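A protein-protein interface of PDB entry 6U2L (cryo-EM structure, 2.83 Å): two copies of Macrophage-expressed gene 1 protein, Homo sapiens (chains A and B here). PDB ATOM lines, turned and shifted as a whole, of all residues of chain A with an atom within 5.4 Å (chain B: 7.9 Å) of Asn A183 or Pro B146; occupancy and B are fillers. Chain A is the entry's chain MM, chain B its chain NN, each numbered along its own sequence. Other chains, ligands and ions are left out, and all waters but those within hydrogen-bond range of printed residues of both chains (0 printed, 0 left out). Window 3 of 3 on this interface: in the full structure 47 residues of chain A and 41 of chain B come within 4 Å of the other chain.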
ATOM      1  N   MET A  42     -26.159  10.780   4.205  1.00  0.00           N
ATOM      2  CA  MET A  42     -25.621  11.780   5.097  1.00  0.00           C
ATOM      3  C   MET A  42     -26.413  13.070   5.025  1.00  0.00           C
ATOM      4  O   MET A  42     -27.535  13.112   4.521  1.00  0.00           O
ATOM      5  CB  MET A  42     -24.164  11.986   4.749  1.00  0.00           C
ATOM      6  CG  MET A  42     -23.348  10.803   5.073  1.00  0.00           C
ATOM      7  SD  MET A  42     -23.410  10.586   6.836  1.00  0.00           S
ATOM      8  CE  MET A  42     -22.545   9.064   6.933  1.00  0.00           C
ATOM      9  N   GLY A  43     -25.836  14.128   5.585  1.00  0.00           N
ATOM     10  CA  GLY A  43     -26.437  15.442   5.492  1.00  0.00           C
ATOM     11  C   GLY A  43     -26.484  15.970   4.072  1.00  0.00           C
ATOM     12  O   GLY A  43     -25.784  15.513   3.172  1.00  0.00           O
ATOM     13  N   GLU A 157     -19.183  25.023   6.447  1.00  0.00           N
ATOM     14  CA  GLU A 157     -18.108  24.177   6.932  1.00  0.00           C
ATOM     15  C   GLU A 157     -16.964  24.069   5.943  1.00  0.00           C
ATOM     16  O   GLU A 157     -15.869  23.671   6.338  1.00  0.00           O
ATOM     17  CB  GLU A 157     -18.644  22.794   7.278  1.00  0.00           C
ATOM     18  CG  GLU A 157     -19.683  22.844   8.371  1.00  0.00           C
ATOM     19  CD  GLU A 157     -20.110  21.479   8.856  1.00  0.00           C
ATOM     20  OE1 GLU A 157     -19.586  20.475   8.338  1.00  0.00           O
ATOM     21  OE2 GLU A 157     -20.982  21.412   9.746  1.00  0.00           O
ATOM     22  N   LEU A 179     -13.945  15.898   9.740  1.00  0.00           N
ATOM     23  CA  LEU A 179     -15.293  16.040  10.265  1.00  0.00           C
ATOM     24  C   LEU A 179     -16.304  16.360   9.179  1.00  0.00           C
ATOM     25  O   LEU A 179     -17.504  16.193   9.399  1.00  0.00           O
ATOM     26  CB  LEU A 179     -15.341  17.118  11.342  1.00  0.00           C
ATOM     27  CG  LEU A 179     -15.080  16.704  12.788  1.00  0.00           C
ATOM     28  CD1 LEU A 179     -13.656  16.329  13.043  1.00  0.00           C
ATOM     29  CD2 LEU A 179     -15.486  17.826  13.704  1.00  0.00           C
ATOM     30  N   LEU A 180     -15.845  16.822   8.020  1.00  0.00           N
ATOM     31  CA  LEU A 180     -16.738  16.992   6.887  1.00  0.00           C
ATOM     32  C   LEU A 180     -17.163  15.642   6.332  1.00  0.00           C
ATOM     33  O   LEU A 180     -18.282  15.497   5.839  1.00  0.00           O
ATOM     34  CB  LEU A 180     -16.042  17.811   5.804  1.00  0.00           C
ATOM     35  CG  LEU A 180     -16.878  18.414   4.686  1.00  0.00           C
ATOM     36  CD1 LEU A 180     -17.676  19.593   5.215  1.00  0.00           C
ATOM     37  CD2 LEU A 180     -16.016  18.818   3.530  1.00  0.00           C
ATOM     38  N   VAL A 181     -16.283  14.647   6.419  1.00  0.00           N
ATOM     39  CA  VAL A 181     -16.569  13.312   5.917  1.00  0.00           C
ATOM     40  C   VAL A 181     -17.415  12.528   6.913  1.00  0.00           C
ATOM     41  O   VAL A 181     -18.222  11.685   6.513  1.00  0.00           O
ATOM     42  CB  VAL A 181     -15.233  12.625   5.587  1.00  0.00           C
ATOM     43  CG1 VAL A 181     -15.422  11.229   5.022  1.00  0.00           C
ATOM     44  CG2 VAL A 181     -14.460  13.473   4.614  1.00  0.00           C
ATOM     45  N   LEU A 182     -17.273  12.800   8.212  1.00  0.00           N
ATOM     46  CA  LEU A 182     -18.194  12.237   9.194  1.00  0.00           C
ATOM     47  C   LEU A 182     -19.616  12.717   8.962  1.00  0.00           C
ATOM     48  O   LEU A 182     -20.563  11.943   9.113  1.00  0.00           O
ATOM     49  CB  LEU A 182     -17.759  12.607  10.617  1.00  0.00           C
ATOM     50  CG  LEU A 182     -18.399  11.967  11.867  1.00  0.00           C
ATOM     51  CD1 LEU A 182     -17.435  12.018  12.983  1.00  0.00           C
ATOM     52  CD2 LEU A 182     -19.659  12.629  12.378  1.00  0.00           C
ATOM     53  N   ASN A 183     -19.787  13.980   8.608  1.00  0.00           N
ATOM     54  CA  ASN A 183     -21.115  14.555   8.545  1.00  0.00           C
ATOM     55  C   ASN A 183     -21.733  14.492   7.159  1.00  0.00           C
ATOM     56  O   ASN A 183     -22.960  14.526   7.050  1.00  0.00           O
ATOM     57  CB  ASN A 183     -21.064  16.005   9.018  1.00  0.00           C
ATOM     58  CG  ASN A 183     -20.736  16.123  10.482  1.00  0.00           C
ATOM     59  OD1 ASN A 183     -21.231  15.360  11.301  1.00  0.00           O
ATOM     60  ND2 ASN A 183     -19.892  17.078  10.819  1.00  0.00           N
ATOM     61  N   TYR A 184     -20.927  14.395   6.105  1.00  0.00           N
ATOM     62  CA  TYR A 184     -21.445  14.464   4.751  1.00  0.00           C
ATOM     63  C   TYR A 184     -21.014  13.313   3.858  1.00  0.00           C
ATOM     64  O   TYR A 184     -21.380  13.305   2.685  1.00  0.00           O
ATOM     65  CB  TYR A 184     -21.045  15.790   4.097  1.00  0.00           C
ATOM     66  CG  TYR A 184     -21.681  16.963   4.785  1.00  0.00           C
ATOM     67  CD1 TYR A 184     -22.994  17.304   4.534  1.00  0.00           C
ATOM     68  CD2 TYR A 184     -20.976  17.708   5.713  1.00  0.00           C
ATOM     69  CE1 TYR A 184     -23.580  18.354   5.173  1.00  0.00           C
ATOM     70  CE2 TYR A 184     -21.555  18.762   6.353  1.00  0.00           C
ATOM     71  CZ  TYR A 184     -22.855  19.078   6.078  1.00  0.00           C
ATOM     72  OH  TYR A 184     -23.440  20.133   6.720  1.00  0.00           O
ATOM     73  N   GLY A 185     -20.269  12.352   4.366  1.00  0.00           N
ATOM     74  CA  GLY A 185     -19.964  11.174   3.588  1.00  0.00           C
ATOM     75  C   GLY A 185     -18.822  11.373   2.613  1.00  0.00           C
ATOM     76  O   GLY A 185     -18.038  12.307   2.701  1.00  0.00           O
ATOM     77  N   GLU B  66     -34.192  21.244  12.778  1.00  0.00           N
ATOM     78  CA  GLU B  66     -32.818  20.782  12.681  1.00  0.00           C
ATOM     79  C   GLU B  66     -32.708  19.300  12.367  1.00  0.00           C
ATOM     80  O   GLU B  66     -31.619  18.729  12.463  1.00  0.00           O
ATOM     81  CB  GLU B  66     -32.116  21.050  14.001  1.00  0.00           C
ATOM     82  CG  GLU B  66     -32.763  20.230  15.088  1.00  0.00           C
ATOM     83  CD  GLU B  66     -33.843  20.970  15.814  1.00  0.00           C
ATOM     84  OE1 GLU B  66     -34.125  22.130  15.451  1.00  0.00           O
ATOM     85  OE2 GLU B  66     -34.473  20.346  16.670  1.00  0.00           O
ATOM     86  N   PHE B  68     -33.604  16.086   9.753  1.00  0.00           N
ATOM     87  CA  PHE B  68     -34.059  15.586   8.471  1.00  0.00           C
ATOM     88  C   PHE B  68     -34.343  14.096   8.572  1.00  0.00           C
ATOM     89  O   PHE B  68     -33.712  13.373   9.339  1.00  0.00           O
ATOM     90  CB  PHE B  68     -33.052  15.878   7.357  1.00  0.00           C
ATOM     91  CG  PHE B  68     -31.765  15.128   7.461  1.00  0.00           C
ATOM     92  CD1 PHE B  68     -30.745  15.593   8.257  1.00  0.00           C
ATOM     93  CD2 PHE B  68     -31.539  14.006   6.686  1.00  0.00           C
ATOM     94  CE1 PHE B  68     -29.553  14.917   8.331  1.00  0.00           C
ATOM     95  CE2 PHE B  68     -30.349  13.331   6.759  1.00  0.00           C
ATOM     96  CZ  PHE B  68     -29.355  13.790   7.579  1.00  0.00           C
ATOM     97  N   LYS B 143     -32.368  11.781  11.488  1.00  0.00           N
ATOM     98  CA  LYS B 143     -31.026  12.234  11.834  1.00  0.00           C
ATOM     99  C   LYS B 143     -31.015  13.700  12.239  1.00  0.00           C
ATOM    100  O   LYS B 143     -31.998  14.418  12.092  1.00  0.00           O
ATOM    101  CB  LYS B 143     -30.050  12.044  10.674  1.00  0.00           C
ATOM    102  CG  LYS B 143     -29.752  10.630  10.327  1.00  0.00           C
ATOM    103  CD  LYS B 143     -28.591  10.541   9.377  1.00  0.00           C
ATOM    104  CE  LYS B 143     -28.219   9.107   9.132  1.00  0.00           C
ATOM    105  NZ  LYS B 143     -27.020   8.984   8.271  1.00  0.00           N
ATOM    106  N   ILE B 144     -29.864  14.146  12.735  1.00  0.00           N
ATOM    107  CA  ILE B 144     -29.645  15.531  13.134  1.00  0.00           C
ATOM    108  C   ILE B 144     -28.766  16.232  12.106  1.00  0.00           C
ATOM    109  O   ILE B 144     -27.800  15.659  11.593  1.00  0.00           O
ATOM    110  CB  ILE B 144     -29.033  15.638  14.545  1.00  0.00           C
ATOM    111  CG1 ILE B 144     -27.798  14.760  14.684  1.00  0.00           C
ATOM    112  CG2 ILE B 144     -30.044  15.308  15.604  1.00  0.00           C
ATOM    113  CD1 ILE B 144     -27.080  14.938  15.982  1.00  0.00           C
ATOM    114  N   ASN B 145     -29.143  17.457  11.775  1.00  0.00           N
ATOM    115  CA  ASN B 145     -28.320  18.336  10.960  1.00  0.00           C
ATOM    116  C   ASN B 145     -27.064  18.677  11.753  1.00  0.00           C
ATOM    117  O   ASN B 145     -27.162  18.956  12.949  1.00  0.00           O
ATOM    118  CB  ASN B 145     -29.162  19.577  10.630  1.00  0.00           C
ATOM    119  CG  ASN B 145     -28.574  20.484   9.564  1.00  0.00           C
ATOM    120  OD1 ASN B 145     -27.443  20.341   9.127  1.00  0.00           O
ATOM    121  ND2 ASN B 145     -29.387  21.433   9.121  1.00  0.00           N
ATOM    122  N   PRO B 146     -25.870  18.617  11.152  1.00  0.00           N
ATOM    123  CA  PRO B 146     -24.637  18.898  11.910  1.00  0.00           C
ATOM    124  C   PRO B 146     -24.469  20.329  12.407  1.00  0.00           C
ATOM    125  O   PRO B 146     -23.494  20.597  13.115  1.00  0.00           O
ATOM    126  CB  PRO B 146     -23.536  18.552  10.907  1.00  0.00           C
ATOM    127  CG  PRO B 146     -24.143  17.539  10.046  1.00  0.00           C
ATOM    128  CD  PRO B 146     -25.570  17.905   9.897  1.00  0.00           C
ATOM    129  N   THR B 147     -25.358  21.260  12.075  1.00  0.00           N
ATOM    130  CA  THR B 147     -25.253  22.642  12.534  1.00  0.00           C
ATOM    131  C   THR B 147     -26.260  22.950  13.629  1.00  0.00           C
ATOM    132  O   THR B 147     -26.855  24.027  13.666  1.00  0.00           O
ATOM    133  CB  THR B 147     -25.419  23.599  11.363  1.00  0.00           C
ATOM    134  OG1 THR B 147     -26.713  23.415  10.776  1.00  0.00           O
ATOM    135  CG2 THR B 147     -24.348  23.334  10.323  1.00  0.00           C
ATOM    136  N   LEU B 148     -26.473  22.004  14.525  1.00  0.00           N
ATOM    137  CA  LEU B 148     -27.419  22.123  15.619  1.00  0.00           C
ATOM    138  C   LEU B 148     -26.717  22.612  16.879  1.00  0.00           C
ATOM    139  O   LEU B 148     -25.511  22.433  17.039  1.00  0.00           O
ATOM    140  CB  LEU B 148     -28.095  20.768  15.837  1.00  0.00           C
ATOM    141  CG  LEU B 148     -28.998  20.393  17.003  1.00  0.00           C
ATOM    142  CD1 LEU B 148     -30.111  21.369  17.230  1.00  0.00           C
ATOM    143  CD2 LEU B 148     -29.575  19.046  16.676  1.00  0.00           C
ATOM    144  N   GLU B 149     -27.473  23.273  17.752  1.00  0.00           N
ATOM    145  CA  GLU B 149     -26.973  23.810  19.008  1.00  0.00           C
ATOM    146  C   GLU B 149     -27.533  23.033  20.194  1.00  0.00           C
ATOM    147  O   GLU B 149     -28.503  22.285  20.084  1.00  0.00           O
ATOM    148  CB  GLU B 149     -27.325  25.293  19.141  1.00  0.00           C
ATOM    149  CG  GLU B 149     -28.799  25.561  19.296  1.00  0.00           C
ATOM    150  CD  GLU B 149     -29.111  27.039  19.350  1.00  0.00           C
ATOM    151  OE1 GLU B 149     -28.167  27.847  19.239  1.00  0.00           O
ATOM    152  OE2 GLU B 149     -30.298  27.395  19.496  1.00  0.00           O
ATOM    153  N   THR B 190     -27.461  10.245  17.625  1.00  0.00           N
ATOM    154  CA  THR B 190     -27.437  11.094  16.450  1.00  0.00           C
ATOM    155  C   THR B 190     -28.347  10.602  15.341  1.00  0.00           C
ATOM    156  O   THR B 190     -28.726  11.397  14.481  1.00  0.00           O
ATOM    157  CB  THR B 190     -26.010  11.236  15.910  1.00  0.00           C
ATOM    158  OG1 THR B 190     -25.505   9.957  15.534  1.00  0.00           O
ATOM    159  CG2 THR B 190     -25.116  11.822  16.963  1.00  0.00           C
ATOM    160  N   LEU B 291     -22.741   9.079  19.312  1.00  0.00           N
ATOM    161  CA  LEU B 291     -21.384   9.533  19.562  1.00  0.00           C
ATOM    162  C   LEU B 291     -21.258   9.769  21.055  1.00  0.00           C
ATOM    163  O   LEU B 291     -22.268   9.978  21.735  1.00  0.00           O
ATOM    164  CB  LEU B 291     -21.076  10.812  18.775  1.00  0.00           C
ATOM    165  CG  LEU B 291     -20.883  10.613  17.276  1.00  0.00           C
ATOM    166  CD1 LEU B 291     -20.888  11.924  16.552  1.00  0.00           C
ATOM    167  CD2 LEU B 291     -19.576   9.896  17.045  1.00  0.00           C
ATOM    168  N   PHE B 295     -17.867  14.458  22.719  1.00  0.00           N
ATOM    169  CA  PHE B 295     -17.695  14.882  21.337  1.00  0.00           C
ATOM    170  C   PHE B 295     -18.365  16.224  21.089  1.00  0.00           C
ATOM    171  O   PHE B 295     -17.878  17.024  20.287  1.00  0.00           O
ATOM    172  CB  PHE B 295     -18.273  13.823  20.402  1.00  0.00           C
ATOM    173  CG  PHE B 295     -18.072  14.110  18.948  1.00  0.00           C
ATOM    174  CD1 PHE B 295     -16.874  13.807  18.334  1.00  0.00           C
ATOM    175  CD2 PHE B 295     -19.079  14.687  18.189  1.00  0.00           C
ATOM    176  CE1 PHE B 295     -16.683  14.070  16.994  1.00  0.00           C
ATOM    177  CE2 PHE B 295     -18.887  14.960  16.849  1.00  0.00           C
ATOM    178  CZ  PHE B 295     -17.690  14.642  16.254  1.00  0.00           C
ATOM    179  N   PHE B 296     -19.471  16.485  21.769  1.00  0.00           N
ATOM    180  CA  PHE B 296     -20.255  17.685  21.567  1.00  0.00           C
ATOM    181  C   PHE B 296     -19.869  18.796  22.524  1.00  0.00           C
ATOM    182  O   PHE B 296     -20.594  19.785  22.633  1.00  0.00           O
ATOM    183  CB  PHE B 296     -21.736  17.349  21.699  1.00  0.00           C
ATOM    184  CG  PHE B 296     -22.207  16.358  20.686  1.00  0.00           C
ATOM    185  CD1 PHE B 296     -22.503  16.754  19.399  1.00  0.00           C
ATOM    186  CD2 PHE B 296     -22.312  15.020  21.007  1.00  0.00           C
ATOM    187  CE1 PHE B 296     -22.928  15.839  18.465  1.00  0.00           C
ATOM    188  CE2 PHE B 296     -22.722  14.106  20.077  1.00  0.00           C
ATOM    189  CZ  PHE B 296     -23.032  14.514  18.806  1.00  0.00           C
ATOM    190  N   ASN B 300     -17.136  24.947  18.952  1.00  0.00           N
ATOM    191  CA  ASN B 300     -18.231  25.299  18.061  1.00  0.00           C
ATOM    192  C   ASN B 300     -19.565  25.324  18.801  1.00  0.00           C
ATOM    193  O   ASN B 300     -20.367  26.241  18.599  1.00  0.00           O
ATOM    194  CB  ASN B 300     -18.272  24.308  16.903  1.00  0.00           C
ATOM    195  CG  ASN B 300     -19.096  24.801  15.742  1.00  0.00           C
ATOM    196  OD1 ASN B 300     -19.607  25.918  15.757  1.00  0.00           O
ATOM    197  ND2 ASN B 300     -19.233  23.966  14.720  1.00  0.00           N
ATOM    198  N   MET B 301     -19.817  24.330  19.661  1.00  0.00           N
ATOM    199  CA  MET B 301     -21.081  24.283  20.392  1.00  0.00           C
ATOM    200  C   MET B 301     -21.154  25.337  21.484  1.00  0.00           C
ATOM    201  O   MET B 301     -22.250  25.749  21.872  1.00  0.00           O
ATOM    202  CB  MET B 301     -21.300  22.908  21.020  1.00  0.00           C
ATOM    203  CG  MET B 301     -21.576  21.791  20.043  1.00  0.00           C
ATOM    204  SD  MET B 301     -23.079  22.007  19.103  1.00  0.00           S
ATOM    205  CE  MET B 301     -22.941  20.597  18.031  1.00  0.00           C
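The backbone carbonyl oxygen of Asn A183 sits at hydrogen-bond distance from the backbone NH of Gly A43 (3.3 Å).
The side-chain amide nitrogen (ND2) of Asn A183 sits at hydrogen-bond distance from the backbone carbonyl oxygen (O) of Leu A179 (2.9 Å).
The backbone NH (N) of Lys B143 sits at hydrogen-bond distance from the backbone carbonyl oxygen (O) of Phe B68.
Phe B68 touches Met A42 (CE2 to O, 3.6 Å).
Gly A43 touches Phe B68.
Thr B147 touches Glu A157 (CG2 to OE2, 3.9 Å).
CB of Asn A183 touches CG of Pro B146, 3.6 Å away.
Asn A183 touches one residue of chain B.
Of the printed residues of chain A, Pro B146 touches Asn A183 (3.6 Å).
Of the printed residues of chain B, Gly A43 touches Phe B68.
Printed residues of chain A within 4 Å of Phe B68: Met A42 and Gly A43.
Of the printed residues of chain A, Thr B147 touches Glu A157 (3.9 Å).
Tyr A184 touches none of the printed residues of chain B.
The nearest printed residue of chain A that does not touch Pro B146 is Glu A157 (4.01 Å).
Of the 15 printed residues of chain B, 3 touch a printed residue of chain A.
Among the printed residues, 4 pairs touch across the chains.
Among the printed residues, no Asp or Glu carboxylate lies within 4 Å of a Lys or Arg side-chain nitrogen of the other chain.
No position is printed for both chains.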
